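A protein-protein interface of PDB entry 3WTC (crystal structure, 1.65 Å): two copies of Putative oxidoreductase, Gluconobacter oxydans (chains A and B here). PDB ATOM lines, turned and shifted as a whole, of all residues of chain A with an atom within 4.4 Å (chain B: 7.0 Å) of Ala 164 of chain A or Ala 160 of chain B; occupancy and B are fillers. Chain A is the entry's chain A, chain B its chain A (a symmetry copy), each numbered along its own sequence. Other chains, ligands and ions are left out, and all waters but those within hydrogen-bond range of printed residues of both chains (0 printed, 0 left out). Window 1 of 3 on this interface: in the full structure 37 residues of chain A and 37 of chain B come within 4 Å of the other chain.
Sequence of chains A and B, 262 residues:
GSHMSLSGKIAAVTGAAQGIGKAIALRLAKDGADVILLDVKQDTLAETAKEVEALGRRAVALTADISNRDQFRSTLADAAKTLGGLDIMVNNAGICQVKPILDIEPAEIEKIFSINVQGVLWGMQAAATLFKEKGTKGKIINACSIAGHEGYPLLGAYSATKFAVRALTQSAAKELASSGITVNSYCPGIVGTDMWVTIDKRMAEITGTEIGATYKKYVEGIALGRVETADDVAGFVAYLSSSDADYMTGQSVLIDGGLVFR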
ATOM      1  N   VAL A 117      18.077  21.700  18.756  1.00  0.00           N
ATOM      2  CA  VAL A 117      16.979  22.076  19.610  1.00  0.00           C
ATOM      3  C   VAL A 117      17.523  22.833  20.820  1.00  0.00           C
ATOM      4  O   VAL A 117      17.139  23.981  21.017  1.00  0.00           O
ATOM      5  CB  VAL A 117      16.207  20.888  20.054  1.00  0.00           C
ATOM      6  CG1 VAL A 117      15.011  21.366  20.896  1.00  0.00           C
ATOM      7  CG2 VAL A 117      15.647  20.157  18.822  1.00  0.00           C
ATOM      8  N   ALA A 160      12.356  15.836  13.231  1.00  0.00           N
ATOM      9  CA  ALA A 160      11.996  15.948  14.628  1.00  0.00           C
ATOM     10  C   ALA A 160      12.590  17.195  15.286  1.00  0.00           C
ATOM     11  O   ALA A 160      11.894  17.887  16.042  1.00  0.00           O
ATOM     12  CB  ALA A 160      12.398  14.685  15.371  1.00  0.00           C
ATOM     13  N   THR A 161      13.872  17.518  15.006  1.00  0.00           N
ATOM     14  CA  THR A 161      14.447  18.683  15.581  1.00  0.00           C
ATOM     15  C   THR A 161      13.776  19.960  15.040  1.00  0.00           C
ATOM     16  O   THR A 161      13.623  20.933  15.789  1.00  0.00           O
ATOM     17  CB  THR A 161      15.968  18.794  15.403  1.00  0.00           C
ATOM     18  OG1 THR A 161      16.370  19.063  14.040  1.00  0.00           O
ATOM     19  CG2 THR A 161      16.698  17.582  15.984  1.00  0.00           C
ATOM     20  N   LYS A 162      13.448  19.977  13.751  1.00  0.00           N
ATOM     21  CA  LYS A 162      12.841  21.198  13.151  1.00  0.00           C
ATOM     22  C   LYS A 162      11.395  21.421  13.582  1.00  0.00           C
ATOM     23  O   LYS A 162      10.979  22.547  13.818  1.00  0.00           O
ATOM     24  CB  LYS A 162      13.064  21.243  11.652  1.00  0.00           C
ATOM     25  CG  LYS A 162      14.520  21.363  11.282  1.00  0.00           C
ATOM     26  CD  LYS A 162      15.232  22.557  11.960  1.00  0.00           C
ATOM     27  CE  LYS A 162      16.633  22.936  11.480  1.00  0.00           C
ATOM     28  NZ  LYS A 162      17.139  24.151  12.170  1.00  0.00           N
ATOM     29  N   PHE A 163      10.650  20.325  13.756  1.00  0.00           N
ATOM     30  CA  PHE A 163       9.325  20.408  14.367  1.00  0.00           C
ATOM     31  C   PHE A 163       9.469  20.986  15.793  1.00  0.00           C
ATOM     32  O   PHE A 163       8.673  21.830  16.210  1.00  0.00           O
ATOM     33  CB  PHE A 163       8.622  19.042  14.426  1.00  0.00           C
ATOM     34  CG  PHE A 163       7.785  18.686  13.218  1.00  0.00           C
ATOM     35  CD1 PHE A 163       8.369  18.381  11.984  1.00  0.00           C
ATOM     36  CD2 PHE A 163       6.386  18.577  13.330  1.00  0.00           C
ATOM     37  CE1 PHE A 163       7.570  17.996  10.944  1.00  0.00           C
ATOM     38  CE2 PHE A 163       5.593  18.181  12.292  1.00  0.00           C
ATOM     39  CZ  PHE A 163       6.211  17.887  11.068  1.00  0.00           C
ATOM     40  N   ALA A 164      10.433  20.468  16.537  1.00  0.00           N
ATOM     41  CA  ALA A 164      10.726  20.968  17.907  1.00  0.00           C
ATOM     42  C   ALA A 164      11.022  22.463  17.882  1.00  0.00           C
ATOM     43  O   ALA A 164      10.568  23.200  18.758  1.00  0.00           O
ATOM     44  CB  ALA A 164      11.777  20.176  18.594  1.00  0.00           C
ATOM     45  N   VAL A 165      11.828  22.941  16.964  1.00  0.00           N
ATOM     46  CA  VAL A 165      12.122  24.342  16.797  1.00  0.00           C
ATOM     47  C   VAL A 165      10.835  25.160  16.583  1.00  0.00           C
ATOM     48  O   VAL A 165      10.651  26.223  17.166  1.00  0.00           O
ATOM     49  CB  VAL A 165      13.187  24.615  15.700  1.00  0.00           C
ATOM     50  CG1 VAL A 165      13.220  26.110  15.339  1.00  0.00           C
ATOM     51  CG2 VAL A 165      14.536  24.140  16.152  1.00  0.00           C
ATOM     52  N   ARG A 166       9.944  24.689  15.739  1.00  0.00           N
ATOM     53  CA  ARG A 166       8.625  25.358  15.526  1.00  0.00           C
ATOM     54  C   ARG A 166       7.811  25.412  16.808  1.00  0.00           C
ATOM     55  O   ARG A 166       7.270  26.473  17.144  1.00  0.00           O
ATOM     56  CB  ARG A 166       7.794  24.656  14.434  1.00  0.00           C
ATOM     57  CG  ARG A 166       8.238  24.571  13.043  1.00  0.00           C
ATOM     58  CD  ARG A 166       7.336  23.507  12.233  1.00  0.00           C
ATOM     59  NE  ARG A 166       5.945  23.789  12.255  1.00  0.00           N
ATOM     60  CZ  ARG A 166       4.879  23.040  12.392  1.00  0.00           C
ATOM     61  NH1 ARG A 166       4.787  21.698  12.295  1.00  0.00           N
ATOM     62  NH2 ARG A 166       3.730  23.724  12.573  1.00  0.00           N
ATOM     63  N   ALA A 167       7.829  24.333  17.598  1.00  0.00           N
ATOM     64  CA  ALA A 167       7.130  24.348  18.899  1.00  0.00           C
ATOM     65  C   ALA A 167       7.721  25.428  19.774  1.00  0.00           C
ATOM     66  O   ALA A 167       6.969  26.163  20.442  1.00  0.00           O
ATOM     67  CB  ALA A 167       7.232  23.030  19.569  1.00  0.00           C
ATOM     68  N   LEU A 168       9.036  25.463  19.892  1.00  0.00           N
ATOM     69  CA  LEU A 168       9.688  26.419  20.810  1.00  0.00           C
ATOM     70  C   LEU A 168       9.441  27.872  20.318  1.00  0.00           C
ATOM     71  O   LEU A 168       9.293  28.782  21.105  1.00  0.00           O
ATOM     72  CB  LEU A 168      11.201  26.159  20.881  1.00  0.00           C
ATOM     73  CG  LEU A 168      11.641  24.838  21.554  1.00  0.00           C
ATOM     74  CD1 LEU A 168      13.141  24.780  21.316  1.00  0.00           C
ATOM     75  CD2 LEU A 168      11.240  24.828  22.998  1.00  0.00           C
ATOM     76  N   ILE B 109      15.704  19.488  30.036  1.00  0.00           N
ATOM     77  CA  ILE B 109      15.276  19.299  28.649  1.00  0.00           C
ATOM     78  C   ILE B 109      15.826  17.964  28.154  1.00  0.00           C
ATOM     79  O   ILE B 109      15.182  17.287  27.400  1.00  0.00           O
ATOM     80  CB  ILE B 109      15.595  20.481  27.767  1.00  0.00           C
ATOM     81  CG1 ILE B 109      14.782  20.330  26.453  1.00  0.00           C
ATOM     82  CG2 ILE B 109      17.066  20.635  27.553  1.00  0.00           C
ATOM     83  CD1 ILE B 109      14.764  21.604  25.687  1.00  0.00           C
ATOM     84  N   PHE B 113      13.345  14.951  26.581  1.00  0.00           N
ATOM     85  CA  PHE B 113      13.579  14.406  25.257  1.00  0.00           C
ATOM     86  C   PHE B 113      13.927  12.908  25.301  1.00  0.00           C
ATOM     87  O   PHE B 113      13.527  12.117  24.461  1.00  0.00           O
ATOM     88  CB  PHE B 113      14.569  15.228  24.490  1.00  0.00           C
ATOM     89  CG  PHE B 113      13.907  16.404  23.754  1.00  0.00           C
ATOM     90  CD1 PHE B 113      13.533  17.528  24.403  1.00  0.00           C
ATOM     91  CD2 PHE B 113      13.508  16.245  22.451  1.00  0.00           C
ATOM     92  CE1 PHE B 113      12.874  18.600  23.754  1.00  0.00           C
ATOM     93  CE2 PHE B 113      12.840  17.273  21.787  1.00  0.00           C
ATOM     94  CZ  PHE B 113      12.560  18.440  22.425  1.00  0.00           C
ATOM     95  N   VAL B 117      10.824  11.569  23.338  1.00  0.00           N
ATOM     96  CA  VAL B 117      11.177  11.482  21.943  1.00  0.00           C
ATOM     97  C   VAL B 117      11.978  10.203  21.709  1.00  0.00           C
ATOM     98  O   VAL B 117      11.543   9.373  20.918  1.00  0.00           O
ATOM     99  CB  VAL B 117      11.961  12.665  21.509  1.00  0.00           C
ATOM    100  CG1 VAL B 117      12.238  12.544  20.000  1.00  0.00           C
ATOM    101  CG2 VAL B 117      11.126  13.938  21.728  1.00  0.00           C
ATOM    102  N   ALA B 147      -0.511  19.709  22.337  1.00  0.00           N
ATOM    103  CA  ALA B 147       0.784  20.465  22.398  1.00  0.00           C
ATOM    104  C   ALA B 147       1.731  19.993  21.320  1.00  0.00           C
ATOM    105  O   ALA B 147       2.838  20.561  21.204  1.00  0.00           O
ATOM    106  CB  ALA B 147       1.362  20.315  23.779  1.00  0.00           C
ATOM    107  N   GLY B 148       1.424  18.919  20.570  1.00  0.00           N
ATOM    108  CA  GLY B 148       2.202  18.564  19.369  1.00  0.00           C
ATOM    109  C   GLY B 148       1.723  19.240  18.111  1.00  0.00           C
ATOM    110  O   GLY B 148       2.336  19.043  17.029  1.00  0.00           O
ATOM    111  N   GLY B 151       2.329  25.155  20.134  1.00  0.00           N
ATOM    112  CA  GLY B 151       3.163  25.359  21.327  1.00  0.00           C
ATOM    113  C   GLY B 151       2.366  26.119  22.404  1.00  0.00           C
ATOM    114  O   GLY B 151       1.700  27.090  22.085  1.00  0.00           O
ATOM    115  N   LEU B 155       4.787  25.264  28.538  1.00  0.00           N
ATOM    116  CA  LEU B 155       4.882  23.905  28.078  1.00  0.00           C
ATOM    117  C   LEU B 155       5.795  23.829  26.879  1.00  0.00           C
ATOM    118  O   LEU B 155       5.620  22.962  26.022  1.00  0.00           O
ATOM    119  CB  LEU B 155       3.500  23.307  27.680  1.00  0.00           C
ATOM    120  CG  LEU B 155       2.563  23.161  28.896  1.00  0.00           C
ATOM    121  CD1 LEU B 155       1.174  22.624  28.441  1.00  0.00           C
ATOM    122  CD2 LEU B 155       3.140  22.225  29.921  1.00  0.00           C
ATOM    123  N   GLY B 156       6.799  24.693  26.822  1.00  0.00           N
ATOM    124  CA  GLY B 156       7.782  24.720  25.701  1.00  0.00           C
ATOM    125  C   GLY B 156       8.482  23.393  25.504  1.00  0.00           C
ATOM    126  O   GLY B 156       8.526  22.840  24.336  1.00  0.00           O
ATOM    127  N   ALA B 157       9.030  22.838  26.579  1.00  0.00           N
ATOM    128  CA  ALA B 157       9.754  21.620  26.437  1.00  0.00           C
ATOM    129  C   ALA B 157       8.810  20.491  26.012  1.00  0.00           C
ATOM    130  O   ALA B 157       9.099  19.698  25.091  1.00  0.00           O
ATOM    131  CB  ALA B 157      10.466  21.234  27.697  1.00  0.00           C
ATOM    132  N   TYR B 158       7.680  20.328  26.747  1.00  0.00           N
ATOM    133  CA  TYR B 158       6.692  19.265  26.416  1.00  0.00           C
ATOM    134  C   TYR B 158       6.183  19.402  24.949  1.00  0.00           C
ATOM    135  O   TYR B 158       6.178  18.416  24.187  1.00  0.00           O
ATOM    136  CB  TYR B 158       5.526  19.382  27.365  1.00  0.00           C
ATOM    137  CG  TYR B 158       4.449  18.329  27.171  1.00  0.00           C
ATOM    138  CD1 TYR B 158       4.652  17.003  27.580  1.00  0.00           C
ATOM    139  CD2 TYR B 158       3.236  18.663  26.581  1.00  0.00           C
ATOM    140  CE1 TYR B 158       3.680  16.015  27.379  1.00  0.00           C
ATOM    141  CE2 TYR B 158       2.286  17.687  26.365  1.00  0.00           C
ATOM    142  CZ  TYR B 158       2.484  16.410  26.781  1.00  0.00           C
ATOM    143  OH  TYR B 158       1.499  15.447  26.573  1.00  0.00           O
ATOM    144  N   SER B 159       5.851  20.628  24.576  1.00  0.00           N
ATOM    145  CA  SER B 159       5.344  20.875  23.213  1.00  0.00           C
ATOM    146  C   SER B 159       6.408  20.487  22.197  1.00  0.00           C
ATOM    147  O   SER B 159       6.148  19.830  21.203  1.00  0.00           O
ATOM    148  CB  SER B 159       4.967  22.345  23.000  1.00  0.00           C
ATOM    149  OG  SER B 159       3.893  22.759  23.837  1.00  0.00           O
ATOM    150  N   ALA B 160       7.654  20.882  22.414  1.00  0.00           N
ATOM    151  CA  ALA B 160       8.741  20.488  21.545  1.00  0.00           C
ATOM    152  C   ALA B 160       8.848  18.970  21.396  1.00  0.00           C
ATOM    153  O   ALA B 160       9.047  18.470  20.279  1.00  0.00           O
ATOM    154  CB  ALA B 160      10.046  21.089  22.040  1.00  0.00           C
ATOM    155  N   THR B 161       8.704  18.206  22.500  1.00  0.00           N
ATOM    156  CA  THR B 161       8.772  16.790  22.393  1.00  0.00           C
ATOM    157  C   THR B 161       7.584  16.235  21.585  1.00  0.00           C
ATOM    158  O   THR B 161       7.752  15.256  20.847  1.00  0.00           O
ATOM    159  CB  THR B 161       8.860  16.055  23.737  1.00  0.00           C
ATOM    160  OG1 THR B 161       7.634  16.106  24.503  1.00  0.00           O
ATOM    161  CG2 THR B 161      10.065  16.517  24.559  1.00  0.00           C
ATOM    162  N   LYS B 162       6.397  16.805  21.775  1.00  0.00           N
ATOM    163  CA  LYS B 162       5.196  16.286  21.064  1.00  0.00           C
ATOM    164  C   LYS B 162       5.187  16.628  19.578  1.00  0.00           C
ATOM    165  O   LYS B 162       4.790  15.818  18.752  1.00  0.00           O
ATOM    166  CB  LYS B 162       3.922  16.649  21.801  1.00  0.00           C
ATOM    167  CG  LYS B 162       3.827  16.002  23.158  1.00  0.00           C
ATOM    168  CD  LYS B 162       3.998  14.464  23.120  1.00  0.00           C
ATOM    169  CE  LYS B 162       3.678  13.666  24.385  1.00  0.00           C
ATOM    170  NZ  LYS B 162       3.810  12.203  24.157  1.00  0.00           N
ATOM    171  N   PHE B 163       5.701  17.813  19.235  1.00  0.00           N
ATOM    172  CA  PHE B 163       5.936  18.154  17.834  1.00  0.00           C
ATOM    173  C   PHE B 163       6.930  17.134  17.233  1.00  0.00           C
ATOM    174  O   PHE B 163       6.746  16.670  16.106  1.00  0.00           O
ATOM    175  CB  PHE B 163       6.484  19.580  17.662  1.00  0.00           C
ATOM    176  CG  PHE B 163       5.441  20.664  17.507  1.00  0.00           C
ATOM    177  CD1 PHE B 163       4.628  21.059  18.575  1.00  0.00           C
ATOM    178  CD2 PHE B 163       5.318  21.364  16.293  1.00  0.00           C
ATOM    179  CE1 PHE B 163       3.751  22.093  18.401  1.00  0.00           C
ATOM    180  CE2 PHE B 163       4.451  22.404  16.126  1.00  0.00           C
ATOM    181  CZ  PHE B 163       3.647  22.770  17.216  1.00  0.00           C
ATOM    182  N   ALA B 164       8.000  16.863  17.965  1.00  0.00           N
ATOM    183  CA  ALA B 164       9.009  15.857  17.540  1.00  0.00           C
ATOM    184  C   ALA B 164       8.353  14.502  17.303  1.00  0.00           C
ATOM    185  O   ALA B 164       8.683  13.814  16.336  1.00  0.00           O
ATOM    186  CB  ALA B 164      10.173  15.790  18.459  1.00  0.00           C
ATOM    187  N   VAL B 165       7.493  14.045  18.182  1.00  0.00           N
ATOM    188  CA  VAL B 165       6.757  12.815  18.028  1.00  0.00           C
ATOM    189  C   VAL B 165       5.945  12.812  16.720  1.00  0.00           C
ATOM    190  O   VAL B 165       5.922  11.829  15.987  1.00  0.00           O
ATOM    191  CB  VAL B 165       5.887  12.467  19.267  1.00  0.00           C
ATOM    192  CG1 VAL B 165       4.889  11.346  18.928  1.00  0.00           C
ATOM    193  CG2 VAL B 165       6.759  12.080  20.425  1.00  0.00           C
ATOM    194  N   ALA B 167       6.625  14.541  14.019  1.00  0.00           N
ATOM    195  CA  ALA B 167       7.610  14.416  12.924  1.00  0.00           C
ATOM    196  C   ALA B 167       7.981  12.963  12.748  1.00  0.00           C
ATOM    197  O   ALA B 167       8.074  12.483  11.601  1.00  0.00           O
ATOM    198  CB  ALA B 167       8.819  15.225  13.205  1.00  0.00           C
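Ala 160 of chain A touches Ala 164 of chain B, and with the chains exchanged Ala 164 of chain A touches Ala 160 of chain B.
Ala 160 of chain A touches Ala 167 of chain B, and with the chains exchanged Ala 167 of chain A touches Ala 160 of chain B.
Phe 163 of chain A touches its own counterpart, Phe 163 of chain B.
Phe 163 of chain A touches Ala 167 of chain B, and with the chains exchanged Ala 167 of chain A touches Phe 163 of chain B.
Positions printed for both chains: 117, 160, 161, 162, 163, 164, 165 and 167.
Of the 11 pairs that touch across the chains among the printed residues, 7 have their exchanged pair printed and touching as well.
Among the printed residues, pairs that only touch across the chains: Phe 163 of chain A with Phe 163 of chain B, Phe 163 of chain A with Ala 167 of chain B, Ala 167 of chain A with Phe 163 of chain B, Ala 160 of chain A with Ala 167 of chain B, Ala 167 of chain A with Ala 160 of chain B, Leu 168 of chain A with Gly 156 of chain B, Ala 160 of chain A with Ala 164 of chain B, Ala 164 of chain A with Ala 160 of chain B, Ala 167 of chain A with Ser 159 of chain B, Arg 166 of chain A with Phe 163 of chain B and Ala 167 of chain A with Gly 151 of chain B.
Along chain B the printed residues that touch a printed residue of chain A span positions 151 to 167.
Printed residues of chain A that touch a printed residue of chain B: Ala 160, Phe 163, Ala 164, Arg 166, Ala 167 and Leu 168.
Hydrophobic or aromatic side chains of chain A that line the printed part of chain B: Ala 160, Phe 163, Ala 164, Ala 167 and Leu 168.
Among the printed residues, 11 pairs touch across the chains.
The side-chain hydroxyl of Ser 159 of chain B is in hydrogen-bond range of the backbone carbonyl oxygen of Leu 155 of chain B (2.8 Å).
Of the printed residues of chain A, Ala 160 of chain B touches Ala 164 (3.6 Å) and Ala 167 (3.6 Å).
Of the printed residues of chain A, Gly 151 of chain B touches Ala 167 (3.99 Å).
Of the printed residues of chain A, Ala 164 of chain B touches Ala 160 (3.6 Å).
Of the printed residues of chain B, Ala 167 of chain A touches Gly 151 (3.99 Å), Ser 159 (3.7 Å), Ala 160 (3.6 Å) and Phe 163 (3.4 Å).
Printed residues of chain B within 4 Å of Phe 163 of chain A: Phe 163 (3.4 Å) and Ala 167 (3.4 Å).
Ala 157 of chain B touches none of the printed residues of chain A.
Val 165 of chain B touches none of the printed residues of chain A.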
